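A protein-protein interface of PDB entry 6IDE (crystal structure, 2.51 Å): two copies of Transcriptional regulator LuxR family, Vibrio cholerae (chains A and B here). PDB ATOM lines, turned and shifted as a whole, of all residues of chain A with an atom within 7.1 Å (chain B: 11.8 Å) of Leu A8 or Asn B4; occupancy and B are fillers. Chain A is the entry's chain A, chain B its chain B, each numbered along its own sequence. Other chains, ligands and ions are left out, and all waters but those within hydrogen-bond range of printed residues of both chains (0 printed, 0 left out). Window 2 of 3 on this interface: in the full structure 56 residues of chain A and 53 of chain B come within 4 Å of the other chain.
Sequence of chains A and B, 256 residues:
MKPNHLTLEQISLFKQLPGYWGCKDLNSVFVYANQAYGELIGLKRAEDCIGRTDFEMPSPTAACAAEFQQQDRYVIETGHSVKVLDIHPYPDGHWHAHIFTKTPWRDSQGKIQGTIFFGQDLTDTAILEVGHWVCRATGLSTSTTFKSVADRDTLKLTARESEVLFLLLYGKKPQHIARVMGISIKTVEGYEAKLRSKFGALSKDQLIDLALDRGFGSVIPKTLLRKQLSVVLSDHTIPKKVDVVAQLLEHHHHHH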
ATOM      1  N   LEU A   6      20.317  16.181  -3.878  1.00  0.00           N
ATOM      2  CA  LEU A   6      19.115  15.421  -4.172  1.00  0.00           C
ATOM      3  C   LEU A   6      19.298  13.976  -3.716  1.00  0.00           C
ATOM      4  O   LEU A   6      20.377  13.397  -3.859  1.00  0.00           O
ATOM      5  CB  LEU A   6      18.807  15.470  -5.670  1.00  0.00           C
ATOM      6  CG  LEU A   6      18.519  16.840  -6.288  1.00  0.00           C
ATOM      7  CD1 LEU A   6      18.187  16.687  -7.749  1.00  0.00           C
ATOM      8  CD2 LEU A   6      17.390  17.546  -5.550  1.00  0.00           C
ATOM      9  N   THR A   7      18.249  13.397  -3.148  1.00  0.00           N
ATOM     10  CA  THR A   7      18.301  11.967  -2.901  1.00  0.00           C
ATOM     11  C   THR A   7      18.279  11.230  -4.237  1.00  0.00           C
ATOM     12  O   THR A   7      17.979  11.809  -5.289  1.00  0.00           O
ATOM     13  CB  THR A   7      17.142  11.522  -2.001  1.00  0.00           C
ATOM     14  OG1 THR A   7      15.902  11.701  -2.689  1.00  0.00           O
ATOM     15  CG2 THR A   7      17.113  12.335  -0.711  1.00  0.00           C
ATOM     16  N   LEU A   8      18.622   9.942  -4.201  1.00  0.00           N
ATOM     17  CA  LEU A   8      18.685   9.219  -5.465  1.00  0.00           C
ATOM     18  C   LEU A   8      17.305   9.013  -6.076  1.00  0.00           C
ATOM     19  O   LEU A   8      17.201   8.889  -7.305  1.00  0.00           O
ATOM     20  CB  LEU A   8      19.413   7.883  -5.302  1.00  0.00           C
ATOM     21  CG  LEU A   8      20.929   7.965  -5.535  1.00  0.00           C
ATOM     22  CD1 LEU A   8      21.583   8.991  -4.610  1.00  0.00           C
ATOM     23  CD2 LEU A   8      21.600   6.610  -5.368  1.00  0.00           C
ATOM     24  N   GLU A   9      16.241   9.005  -5.265  1.00  0.00           N
ATOM     25  CA  GLU A   9      14.914   8.901  -5.860  1.00  0.00           C
ATOM     26  C   GLU A   9      14.453  10.223  -6.455  1.00  0.00           C
ATOM     27  O   GLU A   9      13.679  10.224  -7.415  1.00  0.00           O
ATOM     28  CB  GLU A   9      13.886   8.403  -4.839  1.00  0.00           C
ATOM     29  CG  GLU A   9      13.562   9.399  -3.757  1.00  0.00           C
ATOM     30  CD  GLU A   9      12.238   9.118  -3.072  1.00  0.00           C
ATOM     31  OE1 GLU A   9      11.484   8.238  -3.550  1.00  0.00           O
ATOM     32  OE2 GLU A   9      11.952   9.778  -2.056  1.00  0.00           O
ATOM     33  N   GLN A  10      14.906  11.354  -5.908  1.00  0.00           N
ATOM     34  CA  GLN A  10      14.659  12.625  -6.585  1.00  0.00           C
ATOM     35  C   GLN A  10      15.435  12.712  -7.890  1.00  0.00           C
ATOM     36  O   GLN A  10      14.975  13.347  -8.839  1.00  0.00           O
ATOM     37  CB  GLN A  10      15.014  13.789  -5.664  1.00  0.00           C
ATOM     38  CG  GLN A  10      14.209  13.756  -4.386  1.00  0.00           C
ATOM     39  CD  GLN A  10      14.796  14.619  -3.312  1.00  0.00           C
ATOM     40  OE1 GLN A  10      16.013  14.760  -3.211  1.00  0.00           O
ATOM     41  NE2 GLN A  10      13.938  15.209  -2.497  1.00  0.00           N
ATOM     42  N   ILE A  11      16.596  12.056  -7.963  1.00  0.00           N
ATOM     43  CA  ILE A  11      17.338  11.991  -9.218  1.00  0.00           C
ATOM     44  C   ILE A  11      16.594  11.135 -10.242  1.00  0.00           C
ATOM     45  O   ILE A  11      16.608  11.432 -11.444  1.00  0.00           O
ATOM     46  CB  ILE A  11      18.763  11.472  -8.954  1.00  0.00           C
ATOM     47  CG1 ILE A  11      19.612  12.556  -8.260  1.00  0.00           C
ATOM     48  CG2 ILE A  11      19.411  10.994 -10.240  1.00  0.00           C
ATOM     49  CD1 ILE A  11      20.781  12.001  -7.448  1.00  0.00           C
ATOM     50  N   SER A  12      15.928  10.065  -9.787  1.00  0.00           N
ATOM     51  CA  SER A  12      15.134   9.253 -10.706  1.00  0.00           C
ATOM     52  C   SER A  12      13.992  10.063 -11.298  1.00  0.00           C
ATOM     53  O   SER A  12      13.613   9.851 -12.455  1.00  0.00           O
ATOM     54  CB  SER A  12      14.597   7.998 -10.008  1.00  0.00           C
ATOM     55  OG  SER A  12      13.370   8.229  -9.320  1.00  0.00           O
ATOM     56  N   LEU A  13      13.448  11.011 -10.534  1.00  0.00           N
ATOM     57  CA  LEU A  13      12.439  11.901 -11.096  1.00  0.00           C
ATOM     58  C   LEU A  13      13.047  12.803 -12.166  1.00  0.00           C
ATOM     59  O   LEU A  13      12.442  13.022 -13.220  1.00  0.00           O
ATOM     60  CB  LEU A  13      11.791  12.717  -9.975  1.00  0.00           C
ATOM     61  CG  LEU A  13      11.061  14.007 -10.350  1.00  0.00           C
ATOM     62  CD1 LEU A  13       9.877  13.726 -11.254  1.00  0.00           C
ATOM     63  CD2 LEU A  13      10.629  14.742  -9.093  1.00  0.00           C
ATOM     64  N   PHE A  14      14.253  13.311 -11.917  1.00  0.00           N
ATOM     65  CA  PHE A  14      14.943  14.160 -12.886  1.00  0.00           C
ATOM     66  C   PHE A  14      15.135  13.449 -14.226  1.00  0.00           C
ATOM     67  O   PHE A  14      14.922  14.044 -15.288  1.00  0.00           O
ATOM     68  CB  PHE A  14      16.276  14.600 -12.281  1.00  0.00           C
ATOM     69  CG  PHE A  14      17.139  15.438 -13.181  1.00  0.00           C
ATOM     70  CD1 PHE A  14      16.901  16.802 -13.331  1.00  0.00           C
ATOM     71  CD2 PHE A  14      18.235  14.873 -13.831  1.00  0.00           C
ATOM     72  CE1 PHE A  14      17.721  17.587 -14.133  1.00  0.00           C
ATOM     73  CE2 PHE A  14      19.062  15.649 -14.644  1.00  0.00           C
ATOM     74  CZ  PHE A  14      18.801  17.006 -14.786  1.00  0.00           C
ATOM     75  N   LYS A  15      15.517  12.171 -14.200  1.00  0.00           N
ATOM     76  CA  LYS A  15      15.721  11.435 -15.446  1.00  0.00           C
ATOM     77  C   LYS A  15      14.419  11.042 -16.127  1.00  0.00           C
ATOM     78  O   LYS A  15      14.428  10.742 -17.326  1.00  0.00           O
ATOM     79  CB  LYS A  15      16.550  10.173 -15.204  1.00  0.00           C
ATOM     80  CG  LYS A  15      17.879  10.429 -14.503  1.00  0.00           C
ATOM     81  CD  LYS A  15      18.727   9.170 -14.447  1.00  0.00           C
ATOM     82  CE  LYS A  15      19.946   9.360 -13.563  1.00  0.00           C
ATOM     83  NZ  LYS A  15      20.699  10.601 -13.893  1.00  0.00           N
ATOM     84  N   PRO B   3      26.786   7.446 -14.349  1.00  0.00           N
ATOM     85  CA  PRO B   3      26.866   8.623 -13.480  1.00  0.00           C
ATOM     86  C   PRO B   3      25.855   8.590 -12.338  1.00  0.00           C
ATOM     87  O   PRO B   3      24.701   8.972 -12.534  1.00  0.00           O
ATOM     88  CB  PRO B   3      26.563   9.779 -14.438  1.00  0.00           C
ATOM     89  CG  PRO B   3      25.764   9.162 -15.538  1.00  0.00           C
ATOM     90  CD  PRO B   3      26.343   7.795 -15.712  1.00  0.00           C
ATOM     91  N   ASN B   4      26.285   8.128 -11.162  1.00  0.00           N
ATOM     92  CA  ASN B   4      25.433   8.136  -9.975  1.00  0.00           C
ATOM     93  C   ASN B   4      25.165   9.545  -9.460  1.00  0.00           C
ATOM     94  O   ASN B   4      24.300   9.719  -8.591  1.00  0.00           O
ATOM     95  CB  ASN B   4      26.073   7.297  -8.860  1.00  0.00           C
ATOM     96  CG  ASN B   4      25.125   6.248  -8.286  1.00  0.00           C
ATOM     97  OD1 ASN B   4      23.909   6.319  -8.465  1.00  0.00           O
ATOM     98  ND2 ASN B   4      25.689   5.269  -7.584  1.00  0.00           N
ATOM     99  N   HIS B   5      25.889  10.542  -9.963  1.00  0.00           N
ATOM    100  CA  HIS B   5      25.755  11.922  -9.526  1.00  0.00           C
ATOM    101  C   HIS B   5      25.412  12.821 -10.705  1.00  0.00           C
ATOM    102  O   HIS B   5      25.872  12.605 -11.832  1.00  0.00           O
ATOM    103  CB  HIS B   5      27.050  12.447  -8.888  1.00  0.00           C
ATOM    104  CG  HIS B   5      27.346  11.888  -7.532  1.00  0.00           C
ATOM    105  ND1 HIS B   5      27.842  10.615  -7.342  1.00  0.00           N
ATOM    106  CD2 HIS B   5      27.254  12.444  -6.301  1.00  0.00           C
ATOM    107  CE1 HIS B   5      28.029  10.407  -6.050  1.00  0.00           C
ATOM    108  NE2 HIS B   5      27.683  11.503  -5.397  1.00  0.00           N
ATOM    109  N   LEU B   6      24.605  13.838 -10.426  1.00  0.00           N
ATOM    110  CA  LEU B   6      24.481  14.983 -11.306  1.00  0.00           C
ATOM    111  C   LEU B   6      25.518  16.023 -10.912  1.00  0.00           C
ATOM    112  O   LEU B   6      25.722  16.284  -9.723  1.00  0.00           O
ATOM    113  CB  LEU B   6      23.084  15.590 -11.210  1.00  0.00           C
ATOM    114  CG  LEU B   6      21.895  14.703 -11.579  1.00  0.00           C
ATOM    115  CD1 LEU B   6      20.592  15.437 -11.292  1.00  0.00           C
ATOM    116  CD2 LEU B   6      21.969  14.265 -13.031  1.00  0.00           C
ATOM    117  N   THR B   7      26.177  16.615 -11.906  1.00  0.00           N
ATOM    118  CA  THR B   7      27.006  17.775 -11.611  1.00  0.00           C
ATOM    119  C   THR B   7      26.125  18.890 -11.055  1.00  0.00           C
ATOM    120  O   THR B   7      24.901  18.886 -11.207  1.00  0.00           O
ATOM    121  CB  THR B   7      27.753  18.261 -12.856  1.00  0.00           C
ATOM    122  OG1 THR B   7      26.838  18.900 -13.753  1.00  0.00           O
ATOM    123  CG2 THR B   7      28.412  17.092 -13.571  1.00  0.00           C
ATOM    124  N   LEU B   8      26.758  19.860 -10.403  1.00  0.00           N
ATOM    125  CA  LEU B   8      25.975  20.920  -9.780  1.00  0.00           C
ATOM    126  C   LEU B   8      25.231  21.769 -10.805  1.00  0.00           C
ATOM    127  O   LEU B   8      24.136  22.259 -10.504  1.00  0.00           O
ATOM    128  CB  LEU B   8      26.880  21.778  -8.894  1.00  0.00           C
ATOM    129  CG  LEU B   8      26.715  21.459  -7.403  1.00  0.00           C
ATOM    130  CD1 LEU B   8      26.969  19.983  -7.132  1.00  0.00           C
ATOM    131  CD2 LEU B   8      27.615  22.329  -6.539  1.00  0.00           C
ATOM    132  N   GLN B  10      23.927  20.714 -13.687  1.00  0.00           N
ATOM    133  CA  GLN B  10      22.731  19.947 -14.025  1.00  0.00           C
ATOM    134  C   GLN B  10      21.682  20.027 -12.923  1.00  0.00           C
ATOM    135  O   GLN B  10      20.482  20.067 -13.216  1.00  0.00           O
ATOM    136  CB  GLN B  10      23.108  18.493 -14.296  1.00  0.00           C
ATOM    137  CG  GLN B  10      24.148  18.350 -15.383  1.00  0.00           C
ATOM    138  CD  GLN B  10      24.858  17.014 -15.342  1.00  0.00           C
ATOM    139  OE1 GLN B  10      24.811  16.300 -14.337  1.00  0.00           O
ATOM    140  NE2 GLN B  10      25.523  16.667 -16.439  1.00  0.00           N
ATOM    141  N   ILE B  11      22.111  20.058 -11.658  1.00  0.00           N
ATOM    142  CA  ILE B  11      21.166  20.191 -10.550  1.00  0.00           C
ATOM    143  C   ILE B  11      20.467  21.543 -10.601  1.00  0.00           C
ATOM    144  O   ILE B  11      19.303  21.663 -10.193  1.00  0.00           O
ATOM    145  CB  ILE B  11      21.896  19.983  -9.208  1.00  0.00           C
ATOM    146  CG1 ILE B  11      22.456  18.567  -9.110  1.00  0.00           C
ATOM    147  CG2 ILE B  11      20.976  20.263  -8.039  1.00  0.00           C
ATOM    148  CD1 ILE B  11      23.367  18.372  -7.936  1.00  0.00           C
ATOM    149  N   PHE B  14      17.534  21.157 -12.727  1.00  0.00           N
ATOM    150  CA  PHE B  14      16.458  20.548 -11.951  1.00  0.00           C
ATOM    151  C   PHE B  14      15.616  21.610 -11.259  1.00  0.00           C
ATOM    152  O   PHE B  14      14.394  21.645 -11.409  1.00  0.00           O
ATOM    153  CB  PHE B  14      17.070  19.578 -10.935  1.00  0.00           C
ATOM    154  CG  PHE B  14      16.067  18.858 -10.071  1.00  0.00           C
ATOM    155  CD1 PHE B  14      15.341  17.783 -10.567  1.00  0.00           C
ATOM    156  CD2 PHE B  14      15.890  19.222  -8.744  1.00  0.00           C
ATOM    157  CE1 PHE B  14      14.445  17.107  -9.774  1.00  0.00           C
ATOM    158  CE2 PHE B  14      14.986  18.551  -7.943  1.00  0.00           C
ATOM    159  CZ  PHE B  14      14.263  17.491  -8.459  1.00  0.00           C
ATOM    160  N   CYS B  23       6.193  14.264  -7.976  1.00  0.00           N
ATOM    161  CA  CYS B  23       5.759  12.882  -8.076  1.00  0.00           C
ATOM    162  C   CYS B  23       5.111  12.441  -6.776  1.00  0.00           C
ATOM    163  O   CYS B  23       5.339  13.016  -5.706  1.00  0.00           O
ATOM    164  CB  CYS B  23       6.912  11.941  -8.438  1.00  0.00           C
ATOM    165  SG  CYS B  23       8.247  11.842  -7.214  1.00  0.00           S
ATOM    166  N   VAL B  31       5.877  12.637  -2.933  1.00  0.00           N
ATOM    167  CA  VAL B  31       7.281  12.327  -2.698  1.00  0.00           C
ATOM    168  C   VAL B  31       8.164  13.545  -2.936  1.00  0.00           C
ATOM    169  O   VAL B  31       9.119  13.779  -2.198  1.00  0.00           O
ATOM    170  CB  VAL B  31       7.708  11.140  -3.589  1.00  0.00           C
ATOM    171  CG1 VAL B  31       9.199  10.935  -3.532  1.00  0.00           C
ATOM    172  CG2 VAL B  31       6.975   9.881  -3.168  1.00  0.00           C
ATOM    173  N   TYR B  32       7.831  14.352  -3.938  1.00  0.00           N
ATOM    174  CA  TYR B  32       8.574  15.574  -4.202  1.00  0.00           C
ATOM    175  C   TYR B  32       7.694  16.552  -4.969  1.00  0.00           C
ATOM    176  O   TYR B  32       6.900  16.152  -5.822  1.00  0.00           O
ATOM    177  CB  TYR B  32       9.853  15.292  -4.998  1.00  0.00           C
ATOM    178  CG  TYR B  32      10.642  16.534  -5.307  1.00  0.00           C
ATOM    179  CD1 TYR B  32      11.512  17.068  -4.370  1.00  0.00           C
ATOM    180  CD2 TYR B  32      10.512  17.185  -6.531  1.00  0.00           C
ATOM    181  CE1 TYR B  32      12.228  18.212  -4.640  1.00  0.00           C
ATOM    182  CE2 TYR B  32      11.234  18.333  -6.811  1.00  0.00           C
ATOM    183  CZ  TYR B  32      12.091  18.839  -5.859  1.00  0.00           C
ATOM    184  OH  TYR B  32      12.820  19.978  -6.107  1.00  0.00           O
ATOM    185  N   TRP B 105       5.610   6.647 -12.866  1.00  0.00           N
ATOM    186  CA  TRP B 105       6.914   6.828 -12.252  1.00  0.00           C
ATOM    187  C   TRP B 105       7.449   5.431 -11.969  1.00  0.00           C
ATOM    188  O   TRP B 105       6.835   4.668 -11.217  1.00  0.00           O
ATOM    189  CB  TRP B 105       6.783   7.663 -10.981  1.00  0.00           C
ATOM    190  CG  TRP B 105       8.054   7.868 -10.249  1.00  0.00           C
ATOM    191  CD1 TRP B 105       9.305   7.894 -10.776  1.00  0.00           C
ATOM    192  CD2 TRP B 105       8.202   8.060  -8.838  1.00  0.00           C
ATOM    193  NE1 TRP B 105      10.226   8.098  -9.780  1.00  0.00           N
ATOM    194  CE2 TRP B 105       9.572   8.201  -8.580  1.00  0.00           C
ATOM    195  CE3 TRP B 105       7.305   8.117  -7.769  1.00  0.00           C
ATOM    196  CZ2 TRP B 105      10.074   8.397  -7.295  1.00  0.00           C
ATOM    197  CZ3 TRP B 105       7.802   8.312  -6.492  1.00  0.00           C
ATOM    198  CH2 TRP B 105       9.174   8.449  -6.267  1.00  0.00           C
ATOM    199  N   ARG B 106       8.571   5.083 -12.585  1.00  0.00           N
ATOM    200  CA  ARG B 106       9.060   3.713 -12.534  1.00  0.00           C
ATOM    201  C   ARG B 106      10.292   3.592 -11.652  1.00  0.00           C
ATOM    202  O   ARG B 106      11.106   4.514 -11.551  1.00  0.00           O
ATOM    203  CB  ARG B 106       9.368   3.184 -13.934  1.00  0.00           C
ATOM    204  CG  ARG B 106       8.126   3.120 -14.790  1.00  0.00           C
ATOM    205  CD  ARG B 106       8.396   2.681 -16.207  1.00  0.00           C
ATOM    206  NE  ARG B 106       7.198   2.849 -17.016  1.00  0.00           N
ATOM    207  CZ  ARG B 106       6.251   1.927 -17.134  1.00  0.00           C
ATOM    208  NH1 ARG B 106       6.374   0.774 -16.498  1.00  0.00           N
ATOM    209  NH2 ARG B 106       5.184   2.161 -17.883  1.00  0.00           N
ATOM    210  N   ASP B 107      10.410   2.431 -11.017  1.00  0.00           N
ATOM    211  CA  ASP B 107      11.509   2.153 -10.107  1.00  0.00           C
ATOM    212  C   ASP B 107      12.729   1.698 -10.903  1.00  0.00           C
ATOM    213  O   ASP B 107      12.731   1.682 -12.137  1.00  0.00           O
ATOM    214  CB  ASP B 107      11.095   1.117  -9.066  1.00  0.00           C
ATOM    215  CG  ASP B 107      11.107  -0.306  -9.608  1.00  0.00           C
ATOM    216  OD1 ASP B 107      10.899  -0.496 -10.826  1.00  0.00           O
ATOM    217  OD2 ASP B 107      11.315  -1.243  -8.805  1.00  0.00           O
ATOM    218  N   SER B 108      13.770   1.279 -10.190  1.00  0.00           N
ATOM    219  CA  SER B 108      15.076   1.041 -10.788  1.00  0.00           C
ATOM    220  C   SER B 108      15.052  -0.157 -11.731  1.00  0.00           C
ATOM    221  O   SER B 108      16.062  -0.464 -12.369  1.00  0.00           O
ATOM    222  CB  SER B 108      16.122   0.840  -9.689  1.00  0.00           C
ATOM    223  OG  SER B 108      17.430   0.845 -10.225  1.00  0.00           O
ATOM    224  N   GLN B 109      13.907  -0.839 -11.831  1.00  0.00           N
ATOM    225  CA  GLN B 109      13.791  -2.024 -12.672  1.00  0.00           C
ATOM    226  C   GLN B 109      12.583  -1.986 -13.602  1.00  0.00           C
ATOM    227  O   GLN B 109      12.297  -2.991 -14.261  1.00  0.00           O
ATOM    228  CB  GLN B 109      13.742  -3.293 -11.812  1.00  0.00           C
ATOM    229  CG  GLN B 109      15.047  -3.618 -11.090  1.00  0.00           C
ATOM    230  CD  GLN B 109      15.082  -3.108  -9.652  1.00  0.00           C
ATOM    231  OE1 GLN B 109      14.568  -2.029  -9.348  1.00  0.00           O
ATOM    232  NE2 GLN B 109      15.687  -3.891  -8.761  1.00  0.00           N
ATOM    233  N   GLN B 113       5.925   2.600  -9.601  1.00  0.00           N
ATOM    234  CA  GLN B 113       5.921   2.933  -8.186  1.00  0.00           C
ATOM    235  C   GLN B 113       5.198   4.242  -7.906  1.00  0.00           C
ATOM    236  O   GLN B 113       5.328   4.780  -6.804  1.00  0.00           O
ATOM    237  CB  GLN B 113       7.353   3.023  -7.648  1.00  0.00           C
ATOM    238  CG  GLN B 113       8.103   4.227  -8.169  1.00  0.00           C
ATOM    239  CD  GLN B 113       9.558   4.204  -7.805  1.00  0.00           C
ATOM    240  OE1 GLN B 113       9.986   3.390  -6.997  1.00  0.00           O
ATOM    241  NE2 GLN B 113      10.335   5.089  -8.415  1.00  0.00           N
ATOM    242  N   ILE B 116       4.090  10.659 -11.968  1.00  0.00           N
ATOM    243  CA  ILE B 116       4.764  11.932 -12.211  1.00  0.00           C
ATOM    244  C   ILE B 116       3.750  12.883 -12.829  1.00  0.00           C
ATOM    245  O   ILE B 116       3.117  12.559 -13.843  1.00  0.00           O
ATOM    246  CB  ILE B 116       5.980  11.768 -13.129  1.00  0.00           C
ATOM    247  CG1 ILE B 116       7.057  10.933 -12.455  1.00  0.00           C
ATOM    248  CG2 ILE B 116       6.558  13.126 -13.496  1.00  0.00           C
ATOM    249  CD1 ILE B 116       8.142  10.550 -13.406  1.00  0.00           C
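The backbone NH (N) of Thr A7 is in hydrogen-bond range of the side-chain amide oxygen (OE1) of Gln A10, at 2.6 Å.
The side-chain hydroxyl of Ser A12 is in hydrogen-bond range of the backbone carbonyl oxygen of Glu A9, at 2.8 Å.
The side-chain amide oxygen (OE1) of Gln B10 lies within hydrogen-bond range of the backbone NH (N) of Thr B7.
The backbone NH (N) of Val B31 is in hydrogen-bond range of the backbone carbonyl oxygen (O) of Cys B23, 2.9 Å away.
The backbone carbonyl oxygen (O) of Tyr B32 is in hydrogen-bond range of the backbone NH (N) of Cys B23, 3.0 Å away.
The backbone carbonyl oxygen (O) of Trp B105 lies within hydrogen-bond range of the backbone NH (N) of Gln B113, 2.8 Å away.
The indole nitrogen (NE1) of Trp B105 sits at hydrogen-bond distance from the side-chain hydroxyl (OG) of Ser A12.
Printed residues of chain B that touch a printed residue of chain A: Asn B4, Leu B6, Gln B10, Phe B14, Val B31, Tyr B32 and Trp B105.
Hydrophobic or aromatic side chains of chain B that line the printed part of chain A: Leu B6, Phe B14, Val B31, Tyr B32 and Trp B105.
Hydrophobic or aromatic side chains of chain A within 4 Å of the printed part of chain B: Leu A6, Leu A8, Leu A13 and Phe A14.
No residue of chain B comes within 4 Å of Thr A7.
Of chain B, only Asn B4 (3.9 Å) comes within 4 Å of Leu A8.
Of chain B, only Val B31 (3.3 Å) and Trp B105 (3.6 Å) come within 4 Å of Glu A9.
Of chain B, only Phe B14 (3.9 Å) and Tyr B32 (3.6 Å) come within 4 Å of Gln A10.
Ser A12 touches just one residue of chain B: Trp B105 (3.2 Å).
Printed residues of chain B within 4 Å of Leu A13: Tyr B32 (3.5 Å).
Of the printed residues of chain B, Phe A14 touches Leu B6 (3.5 Å), Gln B10 (3.8 Å) and Phe B14 (3.3 Å).
Asn B4 touches one residue of chain A.
Of the printed residues of chain A, Gln B10 touches Phe A14 (3.8 Å).
Ile B11 touches none of the printed residues of chain A.
Of the printed residues of chain A, Phe B14 touches Leu A6, Gln A10 and Phe A14.
Printed residues of chain A within 4 Å of Val B31: Glu A9.
Gln B113 touches none of the printed residues of chain A.
The nearest residue of chain B that does not touch Leu A8 is His B5 (6.6 Å).
Leu A6 touches Phe B14, and with the chains exchanged Phe A14 touches Leu B6.
Gln A10 touches Phe B14, and with the chains exchanged Phe A14 touches Gln B10.
Phe A14 touches its own counterpart, Phe B14.
Of the 12 pairs that touch across the chains among the printed residues, 5 have their exchanged pair printed and touching as well.
Leu A8 touches Asn B4 (CD2 to OD1, 3.9 Å).
Glu A9 touches Val B31.
Glu A9 touches Trp B105.
Gln A10 touches Phe B14 (O to CE1, 3.9 Å).
Tyr B32 touches Gln A10 (CD1 to NE2, 3.6 Å).
CD2 of Leu A13 touches CD2 of Tyr B32, at 3.5 Å.
Phe A14 touches Leu B6 (CD2 to CD1, 3.5 Å).
Phe A14 touches Gln B10.
CD1 of Phe A14 touches CD1 of Phe B14 (3.3 Å).
CD2 of Leu B6 touches NZ of Lys A15, at 3.97 Å.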
